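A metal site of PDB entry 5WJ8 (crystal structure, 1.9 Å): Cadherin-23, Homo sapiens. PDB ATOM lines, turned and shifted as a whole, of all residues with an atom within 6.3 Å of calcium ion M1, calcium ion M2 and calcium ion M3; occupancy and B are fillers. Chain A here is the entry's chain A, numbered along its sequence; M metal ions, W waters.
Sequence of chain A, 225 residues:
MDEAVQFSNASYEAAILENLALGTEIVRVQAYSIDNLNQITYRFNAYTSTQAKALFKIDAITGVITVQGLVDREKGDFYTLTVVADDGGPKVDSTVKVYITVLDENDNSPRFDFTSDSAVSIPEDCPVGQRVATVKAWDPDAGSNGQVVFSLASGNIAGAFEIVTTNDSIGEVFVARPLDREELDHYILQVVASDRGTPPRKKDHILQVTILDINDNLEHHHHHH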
ATOM      1  N   GLU A  18      15.010  -4.387 -20.604  1.00  0.00           N
ATOM      2  CA  GLU A  18      15.736  -3.414 -21.437  1.00  0.00           C
ATOM      3  C   GLU A  18      15.778  -3.890 -22.894  1.00  0.00           C
ATOM      4  O   GLU A  18      15.575  -5.072 -23.169  1.00  0.00           O
ATOM      5  CB  GLU A  18      17.158  -3.181 -20.926  1.00  0.00           C
ATOM      6  CG  GLU A  18      18.047  -4.416 -20.816  1.00  0.00           C
ATOM      7  CD  GLU A  18      19.504  -4.050 -20.543  1.00  0.00           C
ATOM      8  OE1 GLU A  18      20.255  -4.887 -19.998  1.00  0.00           O
ATOM      9  OE2 GLU A  18      19.908  -2.917 -20.900  1.00  0.00           O
ATOM     10  N   ASN A  19      16.054  -2.962 -23.802  1.00  0.00           N
ATOM     11  CA  ASN A  19      16.227  -3.211 -25.249  1.00  0.00           C
ATOM     12  C   ASN A  19      14.927  -3.545 -26.021  1.00  0.00           C
ATOM     13  O   ASN A  19      14.969  -3.950 -27.171  1.00  0.00           O
ATOM     14  CB  ASN A  19      17.299  -4.283 -25.539  1.00  0.00           C
ATOM     15  CG  ASN A  19      18.670  -3.936 -24.964  1.00  0.00           C
ATOM     16  OD1 ASN A  19      19.111  -2.774 -25.001  1.00  0.00           O
ATOM     17  ND2 ASN A  19      19.361  -4.936 -24.432  1.00  0.00           N
ATOM     18  N   VAL A  71      15.855   1.893 -24.395  1.00  0.00           N
ATOM     19  CA  VAL A  71      15.821   1.630 -22.968  1.00  0.00           C
ATOM     20  C   VAL A  71      17.012   0.744 -22.582  1.00  0.00           C
ATOM     21  O   VAL A  71      17.094  -0.426 -23.036  1.00  0.00           O
ATOM     22  CB  VAL A  71      14.495   0.965 -22.530  1.00  0.00           C
ATOM     23  CG1 VAL A  71      14.507   0.601 -21.053  1.00  0.00           C
ATOM     24  CG2 VAL A  71      13.334   1.902 -22.797  1.00  0.00           C
ATOM     25  N   ASP A  72      17.938   1.319 -21.792  1.00  0.00           N
ATOM     26  CA  ASP A  72      19.203   0.662 -21.456  1.00  0.00           C
ATOM     27  C   ASP A  72      19.325   0.606 -19.952  1.00  0.00           C
ATOM     28  O   ASP A  72      19.490   1.645 -19.306  1.00  0.00           O
ATOM     29  CB  ASP A  72      20.357   1.428 -22.092  1.00  0.00           C
ATOM     30  CG  ASP A  72      21.724   0.813 -21.827  1.00  0.00           C
ATOM     31  OD1 ASP A  72      21.834  -0.246 -21.172  1.00  0.00           O
ATOM     32  OD2 ASP A  72      22.706   1.427 -22.260  1.00  0.00           O
ATOM     33  N   ARG A  73      19.245  -0.595 -19.375  1.00  0.00           N
ATOM     34  CA  ARG A  73      19.346  -0.748 -17.931  1.00  0.00           C
ATOM     35  C   ARG A  73      20.692  -0.220 -17.408  1.00  0.00           C
ATOM     36  O   ARG A  73      20.771   0.309 -16.299  1.00  0.00           O
ATOM     37  CB  ARG A  73      19.180  -2.211 -17.497  1.00  0.00           C
ATOM     38  CG  ARG A  73      18.892  -2.351 -15.996  1.00  0.00           C
ATOM     39  CD  ARG A  73      19.513  -3.594 -15.415  1.00  0.00           C
ATOM     40  NE  ARG A  73      20.966  -3.562 -15.599  1.00  0.00           N
ATOM     41  CZ  ARG A  73      21.849  -2.994 -14.770  1.00  0.00           C
ATOM     42  NH1 ARG A  73      21.473  -2.440 -13.611  1.00  0.00           N
ATOM     43  NH2 ARG A  73      23.134  -3.019 -15.095  1.00  0.00           N
ATOM     44  N   GLU A  74      21.729  -0.332 -18.227  1.00  0.00           N
ATOM     45  CA  GLU A  74      23.053   0.172 -17.853  1.00  0.00           C
ATOM     46  C   GLU A  74      23.097   1.717 -17.701  1.00  0.00           C
ATOM     47  O   GLU A  74      24.002   2.246 -17.050  1.00  0.00           O
ATOM     48  CB  GLU A  74      24.102  -0.305 -18.857  1.00  0.00           C
ATOM     49  CG  GLU A  74      24.559  -1.741 -18.647  1.00  0.00           C
ATOM     50  CD  GLU A  74      23.469  -2.796 -18.866  1.00  0.00           C
ATOM     51  OE1 GLU A  74      22.893  -2.903 -19.979  1.00  0.00           O
ATOM     52  OE2 GLU A  74      23.185  -3.545 -17.922  1.00  0.00           O
ATOM     53  N   LYS A  75      22.140   2.434 -18.289  1.00  0.00           N
ATOM     54  CA  LYS A  75      22.036   3.901 -18.130  1.00  0.00           C
ATOM     55  C   LYS A  75      20.984   4.347 -17.116  1.00  0.00           C
ATOM     56  O   LYS A  75      20.980   5.491 -16.720  1.00  0.00           O
ATOM     57  CB  LYS A  75      21.726   4.542 -19.490  1.00  0.00           C
ATOM     58  CG  LYS A  75      22.894   4.506 -20.455  1.00  0.00           C
ATOM     59  CD  LYS A  75      22.558   5.223 -21.758  1.00  0.00           C
ATOM     60  CE  LYS A  75      23.653   5.139 -22.822  1.00  0.00           C
ATOM     61  NZ  LYS A  75      25.030   4.846 -22.326  1.00  0.00           N
ATOM     62  N   LEU A 103      14.505  -4.164 -16.176  1.00  0.00           N
ATOM     63  CA  LEU A 103      15.155  -5.406 -15.795  1.00  0.00           C
ATOM     64  C   LEU A 103      16.323  -5.679 -16.726  1.00  0.00           C
ATOM     65  O   LEU A 103      16.290  -5.278 -17.902  1.00  0.00           O
ATOM     66  CB  LEU A 103      14.165  -6.579 -15.946  1.00  0.00           C
ATOM     67  CG  LEU A 103      12.809  -6.472 -15.238  1.00  0.00           C
ATOM     68  CD1 LEU A 103      11.940  -7.698 -15.505  1.00  0.00           C
ATOM     69  CD2 LEU A 103      13.004  -6.317 -13.733  1.00  0.00           C
ATOM     70  N   ASP A 104      17.296  -6.423 -16.212  1.00  0.00           N
ATOM     71  CA  ASP A 104      18.546  -6.677 -16.913  1.00  0.00           C
ATOM     72  C   ASP A 104      18.450  -7.775 -17.962  1.00  0.00           C
ATOM     73  O   ASP A 104      17.843  -8.816 -17.705  1.00  0.00           O
ATOM     74  CB  ASP A 104      19.639  -7.081 -15.915  1.00  0.00           C
ATOM     75  CG  ASP A 104      21.037  -6.972 -16.504  1.00  0.00           C
ATOM     76  OD1 ASP A 104      21.370  -6.000 -17.208  1.00  0.00           O
ATOM     77  OD2 ASP A 104      21.847  -7.865 -16.248  1.00  0.00           O
ATOM     78  N   GLU A 105      19.054  -7.517 -19.114  1.00  0.00           N
ATOM     79  CA  GLU A 105      19.430  -8.527 -20.101  1.00  0.00           C
ATOM     80  C   GLU A 105      20.924  -8.674 -20.103  1.00  0.00           C
ATOM     81  O   GLU A 105      21.671  -7.701 -19.848  1.00  0.00           O
ATOM     82  CB  GLU A 105      18.988  -8.126 -21.502  1.00  0.00           C
ATOM     83  CG  GLU A 105      17.486  -8.343 -21.661  1.00  0.00           C
ATOM     84  CD  GLU A 105      16.990  -8.154 -23.077  1.00  0.00           C
ATOM     85  OE1 GLU A 105      17.689  -7.484 -23.891  1.00  0.00           O
ATOM     86  OE2 GLU A 105      15.879  -8.675 -23.340  1.00  0.00           O
ATOM     87  N   ASN A 106      21.374  -9.876 -20.446  1.00  0.00           N
ATOM     88  CA  ASN A 106      22.798 -10.143 -20.570  1.00  0.00           C
ATOM     89  C   ASN A 106      23.279  -9.652 -21.937  1.00  0.00           C
ATOM     90  O   ASN A 106      23.654 -10.435 -22.816  1.00  0.00           O
ATOM     91  CB  ASN A 106      23.119 -11.617 -20.345  1.00  0.00           C
ATOM     92  CG  ASN A 106      24.588 -11.817 -20.048  1.00  0.00           C
ATOM     93  OD1 ASN A 106      25.247 -10.865 -19.654  1.00  0.00           O
ATOM     94  ND2 ASN A 106      25.121 -13.030 -20.244  1.00  0.00           N
ATOM     95  N   ASP A 107      23.315  -8.335 -22.095  1.00  0.00           N
ATOM     96  CA  ASP A 107      23.546  -7.734 -23.389  1.00  0.00           C
ATOM     97  C   ASP A 107      24.977  -7.217 -23.536  1.00  0.00           C
ATOM     98  O   ASP A 107      25.287  -6.541 -24.498  1.00  0.00           O
ATOM     99  CB  ASP A 107      22.477  -6.684 -23.744  1.00  0.00           C
ATOM    100  CG  ASP A 107      22.396  -5.504 -22.760  1.00  0.00           C
ATOM    101  OD1 ASP A 107      22.843  -5.562 -21.596  1.00  0.00           O
ATOM    102  OD2 ASP A 107      21.789  -4.507 -23.166  1.00  0.00           O
ATOM    103  N   ASN A 108      25.841  -7.591 -22.594  1.00  0.00           N
ATOM    104  CA  ASN A 108      27.263  -7.294 -22.694  1.00  0.00           C
ATOM    105  C   ASN A 108      28.093  -8.529 -22.419  1.00  0.00           C
ATOM    106  O   ASN A 108      27.804  -9.300 -21.495  1.00  0.00           O
ATOM    107  CB  ASN A 108      27.661  -6.173 -21.714  1.00  0.00           C
ATOM    108  CG  ASN A 108      26.957  -4.873 -22.012  1.00  0.00           C
ATOM    109  OD1 ASN A 108      27.470  -4.039 -22.765  1.00  0.00           O
ATOM    110  ND2 ASN A 108      25.763  -4.708 -21.466  1.00  0.00           N
ATOM    111  N   SER A 109      29.134  -8.700 -23.230  1.00  0.00           N
ATOM    112  CA  SER A 109      30.201  -9.655 -22.975  1.00  0.00           C
ATOM    113  C   SER A 109      31.294  -8.953 -22.174  1.00  0.00           C
ATOM    114  O   SER A 109      31.446  -7.741 -22.275  1.00  0.00           O
ATOM    115  CB  SER A 109      30.838 -10.125 -24.285  1.00  0.00           C
ATOM    116  OG  SER A 109      29.893 -10.784 -25.104  1.00  0.00           O
ATOM    117  N   PRO A 110      32.084  -9.724 -21.400  1.00  0.00           N
ATOM    118  CA  PRO A 110      33.285  -9.155 -20.787  1.00  0.00           C
ATOM    119  C   PRO A 110      34.170  -8.504 -21.832  1.00  0.00           C
ATOM    120  O   PRO A 110      34.318  -9.031 -22.924  1.00  0.00           O
ATOM    121  CB  PRO A 110      33.974 -10.388 -20.189  1.00  0.00           C
ATOM    122  CG  PRO A 110      32.855 -11.325 -19.869  1.00  0.00           C
ATOM    123  CD  PRO A 110      31.837 -11.107 -20.958  1.00  0.00           C
ATOM    124  N   ASP A 139      32.393  -6.068 -17.087  1.00  0.00           N
ATOM    125  CA  ASP A 139      31.089  -6.414 -17.624  1.00  0.00           C
ATOM    126  C   ASP A 139      30.058  -5.598 -16.840  1.00  0.00           C
ATOM    127  O   ASP A 139      29.850  -5.867 -15.664  1.00  0.00           O
ATOM    128  CB  ASP A 139      30.858  -7.901 -17.494  1.00  0.00           C
ATOM    129  CG  ASP A 139      29.639  -8.381 -18.265  1.00  0.00           C
ATOM    130  OD1 ASP A 139      28.577  -7.714 -18.222  1.00  0.00           O
ATOM    131  OD2 ASP A 139      29.748  -9.456 -18.904  1.00  0.00           O
ATOM    132  N   PRO A 140      29.389  -4.634 -17.509  1.00  0.00           N
ATOM    133  CA  PRO A 140      28.454  -3.722 -16.854  1.00  0.00           C
ATOM    134  C   PRO A 140      27.048  -4.261 -16.529  1.00  0.00           C
ATOM    135  O   PRO A 140      26.244  -3.520 -15.965  1.00  0.00           O
ATOM    136  CB  PRO A 140      28.335  -2.585 -17.872  1.00  0.00           C
ATOM    137  CG  PRO A 140      28.509  -3.271 -19.188  1.00  0.00           C
ATOM    138  CD  PRO A 140      29.544  -4.301 -18.939  1.00  0.00           C
ATOM    139  N   ASP A 141      26.735  -5.512 -16.866  1.00  0.00           N
ATOM    140  CA  ASP A 141      25.411  -6.063 -16.558  1.00  0.00           C
ATOM    141  C   ASP A 141      25.237  -6.276 -15.040  1.00  0.00           C
ATOM    142  O   ASP A 141      26.201  -6.240 -14.281  1.00  0.00           O
ATOM    143  CB  ASP A 141      25.170  -7.379 -17.318  1.00  0.00           C
ATOM    144  CG  ASP A 141      25.156  -7.188 -18.840  1.00  0.00           C
ATOM    145  OD1 ASP A 141      24.528  -6.246 -19.365  1.00  0.00           O
ATOM    146  OD2 ASP A 141      25.784  -8.026 -19.535  1.00  0.00           O
ATOM    147  N   ALA A 142      24.006  -6.525 -14.610  1.00  0.00           N
ATOM    148  CA  ALA A 142      23.681  -6.710 -13.215  1.00  0.00           C
ATOM    149  C   ALA A 142      23.826  -8.148 -12.760  1.00  0.00           C
ATOM    150  O   ALA A 142      23.739  -9.072 -13.572  1.00  0.00           O
ATOM    151  CB  ALA A 142      22.280  -6.201 -12.916  1.00  0.00           C
ATOM    152  N   SER A 144      24.627 -11.800 -11.613  1.00  0.00           N
ATOM    153  CA  SER A 144      25.382 -12.836 -12.338  1.00  0.00           C
ATOM    154  C   SER A 144      25.802 -12.453 -13.757  1.00  0.00           C
ATOM    155  O   SER A 144      26.915 -12.803 -14.189  1.00  0.00           O
ATOM    156  CB  SER A 144      24.566 -14.122 -12.414  1.00  0.00           C
ATOM    157  OG  SER A 144      24.410 -14.672 -11.123  1.00  0.00           O
ATOM    158  N   ASN A 145      24.949 -11.747 -14.489  1.00  0.00           N
ATOM    159  CA  ASN A 145      25.232 -11.331 -15.870  1.00  0.00           C
ATOM    160  C   ASN A 145      26.494 -10.480 -16.005  1.00  0.00           C
ATOM    161  O   ASN A 145      27.069 -10.432 -17.117  1.00  0.00           O
ATOM    162  CB  ASN A 145      24.068 -10.537 -16.487  1.00  0.00           C
ATOM    163  CG  ASN A 145      22.851 -11.392 -16.799  1.00  0.00           C
ATOM    164  OD1 ASN A 145      22.940 -12.608 -16.929  1.00  0.00           O
ATOM    165  ND2 ASN A 145      21.711 -10.722 -16.966  1.00  0.00           N
ATOM    166  N   GLY A 146      26.854  -9.789 -14.938  1.00  0.00           N
ATOM    167  CA  GLY A 146      28.008  -8.899 -14.908  1.00  0.00           C
ATOM    168  C   GLY A 146      29.187  -9.375 -14.082  1.00  0.00           C
ATOM    169  O   GLY A 146      30.186  -8.681 -13.986  1.00  0.00           O
ATOM    170  N   GLN A 147      29.083 -10.549 -13.469  1.00  0.00           N
ATOM    171  CA  GLN A 147      30.209 -11.178 -12.758  1.00  0.00           C
ATOM    172  C   GLN A 147      31.132 -11.891 -13.723  1.00  0.00           C
ATOM    173  O   GLN A 147      30.654 -12.689 -14.505  1.00  0.00           O
ATOM    174  CB  GLN A 147      29.687 -12.203 -11.754  1.00  0.00           C
ATOM    175  CG  GLN A 147      29.009 -11.527 -10.583  1.00  0.00           C
ATOM    176  CD  GLN A 147      28.399 -12.494  -9.601  1.00  0.00           C
ATOM    177  OE1 GLN A 147      28.045 -13.632  -9.937  1.00  0.00           O
ATOM    178  NE2 GLN A 147      28.242 -12.031  -8.375  1.00  0.00           N
ATOM    179  N   ASP A 195      31.229 -14.241 -18.348  1.00  0.00           N
ATOM    180  CA  ASP A 195      30.284 -13.796 -17.325  1.00  0.00           C
ATOM    181  C   ASP A 195      29.566 -15.024 -16.756  1.00  0.00           C
ATOM    182  O   ASP A 195      29.829 -16.154 -17.182  1.00  0.00           O
ATOM    183  CB  ASP A 195      29.334 -12.682 -17.783  1.00  0.00           C
ATOM    184  CG  ASP A 195      28.353 -13.102 -18.864  1.00  0.00           C
ATOM    185  OD1 ASP A 195      27.956 -14.296 -18.918  1.00  0.00           O
ATOM    186  OD2 ASP A 195      27.972 -12.216 -19.674  1.00  0.00           O
ATOM    187  N   ARG A 196      28.675 -14.832 -15.790  1.00  0.00           N
ATOM    188  CA  ARG A 196      27.870 -15.912 -15.261  1.00  0.00           C
ATOM    189  C   ARG A 196      26.408 -15.805 -15.664  1.00  0.00           C
ATOM    190  O   ARG A 196      25.540 -16.193 -14.911  1.00  0.00           O
ATOM    191  CB  ARG A 196      27.953 -15.958 -13.749  1.00  0.00           C
ATOM    192  CG  ARG A 196      29.346 -16.118 -13.202  1.00  0.00           C
ATOM    193  CD  ARG A 196      29.266 -16.223 -11.690  1.00  0.00           C
ATOM    194  NE  ARG A 196      30.215 -17.207 -11.198  1.00  0.00           N
ATOM    195  CZ  ARG A 196      31.395 -16.950 -10.619  1.00  0.00           C
ATOM    196  NH1 ARG A 196      31.824 -15.693 -10.417  1.00  0.00           N
ATOM    197  NH2 ARG A 196      32.157 -17.968 -10.254  1.00  0.00           N
ATOM    198  N   GLY A 197      26.138 -15.299 -16.862  1.00  0.00           N
ATOM    199  CA  GLY A 197      24.797 -15.388 -17.436  1.00  0.00           C
ATOM    200  C   GLY A 197      24.453 -16.830 -17.792  1.00  0.00           C
ATOM    201  O   GLY A 197      25.308 -17.708 -17.748  1.00  0.00           O
ATOM    202  N   ARG A 201      28.366 -15.451 -21.566  1.00  0.00           N
ATOM    203  CA  ARG A 201      29.003 -14.761 -22.674  1.00  0.00           C
ATOM    204  C   ARG A 201      30.473 -14.706 -22.340  1.00  0.00           C
ATOM    205  O   ARG A 201      30.848 -14.563 -21.166  1.00  0.00           O
ATOM    206  CB  ARG A 201      28.447 -13.357 -22.824  1.00  0.00           C
ATOM    207  CG  ARG A 201      26.966 -13.385 -23.176  1.00  0.00           C
ATOM    208  CD  ARG A 201      26.339 -12.030 -23.416  1.00  0.00           C
ATOM    209  NE  ARG A 201      26.992 -11.265 -24.484  1.00  0.00           N
ATOM    210  CZ  ARG A 201      26.400 -10.387 -25.273  1.00  0.00           C
ATOM    211  NH1 ARG A 201      25.105 -10.077 -25.152  1.00  0.00           N
ATOM    212  NH2 ARG A 201      27.125  -9.789 -26.216  1.00  0.00           N
HETATM  213 CA    CA M   1      22.037  -2.456 -21.909  1.00  0.00          CA
HETATM  214 CA    CA M   2      22.330  -5.422 -19.309  1.00  0.00          CA
HETATM  215 CA    CA M   3      27.376  -9.811 -19.323  1.00  0.00          CA
HETATM  216  O   HOH W   1      21.079  -1.539 -23.818  1.00  0.00           O
HETATM  217  O   HOH W   2      24.221  -2.382 -22.674  1.00  0.00           O
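N of Ala 142 sits at hydrogen-bond distance from OD2 of Asp 104 (3.0 Å).
The side-chain carboxylate (OE2) of Glu 74 lies close to the guanidinium group (NH2) of Arg 73, 2.9 Å away.
The side-chain amide nitrogen of Asn 145 sits at hydrogen-bond distance from the side-chain carboxylate of Asp 104 (2.9 Å).
The side-chain carboxylate of Asp 107 lies close to the side-chain amide nitrogen of Asn 19, at 2.8 Å.
The side-chain carboxylate of Glu 18 sits close to the backbone NH of Arg 73 (2.9 Å).
The backbone carbonyl oxygen (O) of Arg 201 is in hydrogen-bond range of the backbone NH (N) of Asp 195, at 2.9 Å.
OE1 of Glu 105 sits at hydrogen-bond distance from ND2 of Asn 19 (3.1 Å).
N of Glu 18 is in hydrogen-bond range of O of Leu 103 (3.1 Å).
Four residues have an atom within 4 Å of calcium ion M1: Glu 18, Asp 72, Glu 74 and Asp 107.
Along chain A the residues within 4 Å of calcium ion M1 span positions 18 to 107.
The nearest printed residue that does not touch calcium ion M1 is Arg 73 (4.2 Å).
The nearest printed residue that does not touch calcium ion M2 is Asn 108 (4.1 Å).
Of the 27 residues printed, 6 come within 4 Å of calcium ion M3.
The nearest printed residue that does not touch calcium ion M3 is Gly 146 (4.4 Å).
Calcium ion M1 is bound by OE1 of Glu 74 (2.2 Å), water W2 (2.3 Å), water W1 (2.3 Å), OD1 of Asp 72 (2.3 Å), OE2 of Glu 18 (2.4 Å) and OD2 of Asp 107 (2.4 Å).
Calcium ion M2 is bound by the side-chain carboxylate (OE1) of Glu 18 (2.3 Å), the side-chain carboxylate (OD1) of Asp 107 (2.3 Å), the side-chain carboxylate (OD1) of Asp 141 (2.3 Å), the side-chain carboxylate (OD1) of Asp 104 (2.4 Å), the backbone carbonyl oxygen (O) of Glu 105 (2.4 Å), the side-chain carboxylate (OE2) of Glu 74 (2.5 Å) and the side-chain carboxylate (OE1) of Glu 74 (2.7 Å).
Calcium ion M3 is bound by O of Asn 108 (2.3 Å), O of Asn 145 (2.3 Å), OD1 of Asn 106 (2.4 Å), OD2 of Asp 141 (2.4 Å), OD2 of Asp 139 (2.4 Å), OD2 of Asp 195 (2.5 Å) and OD1 of Asp 139 (2.7 Å).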
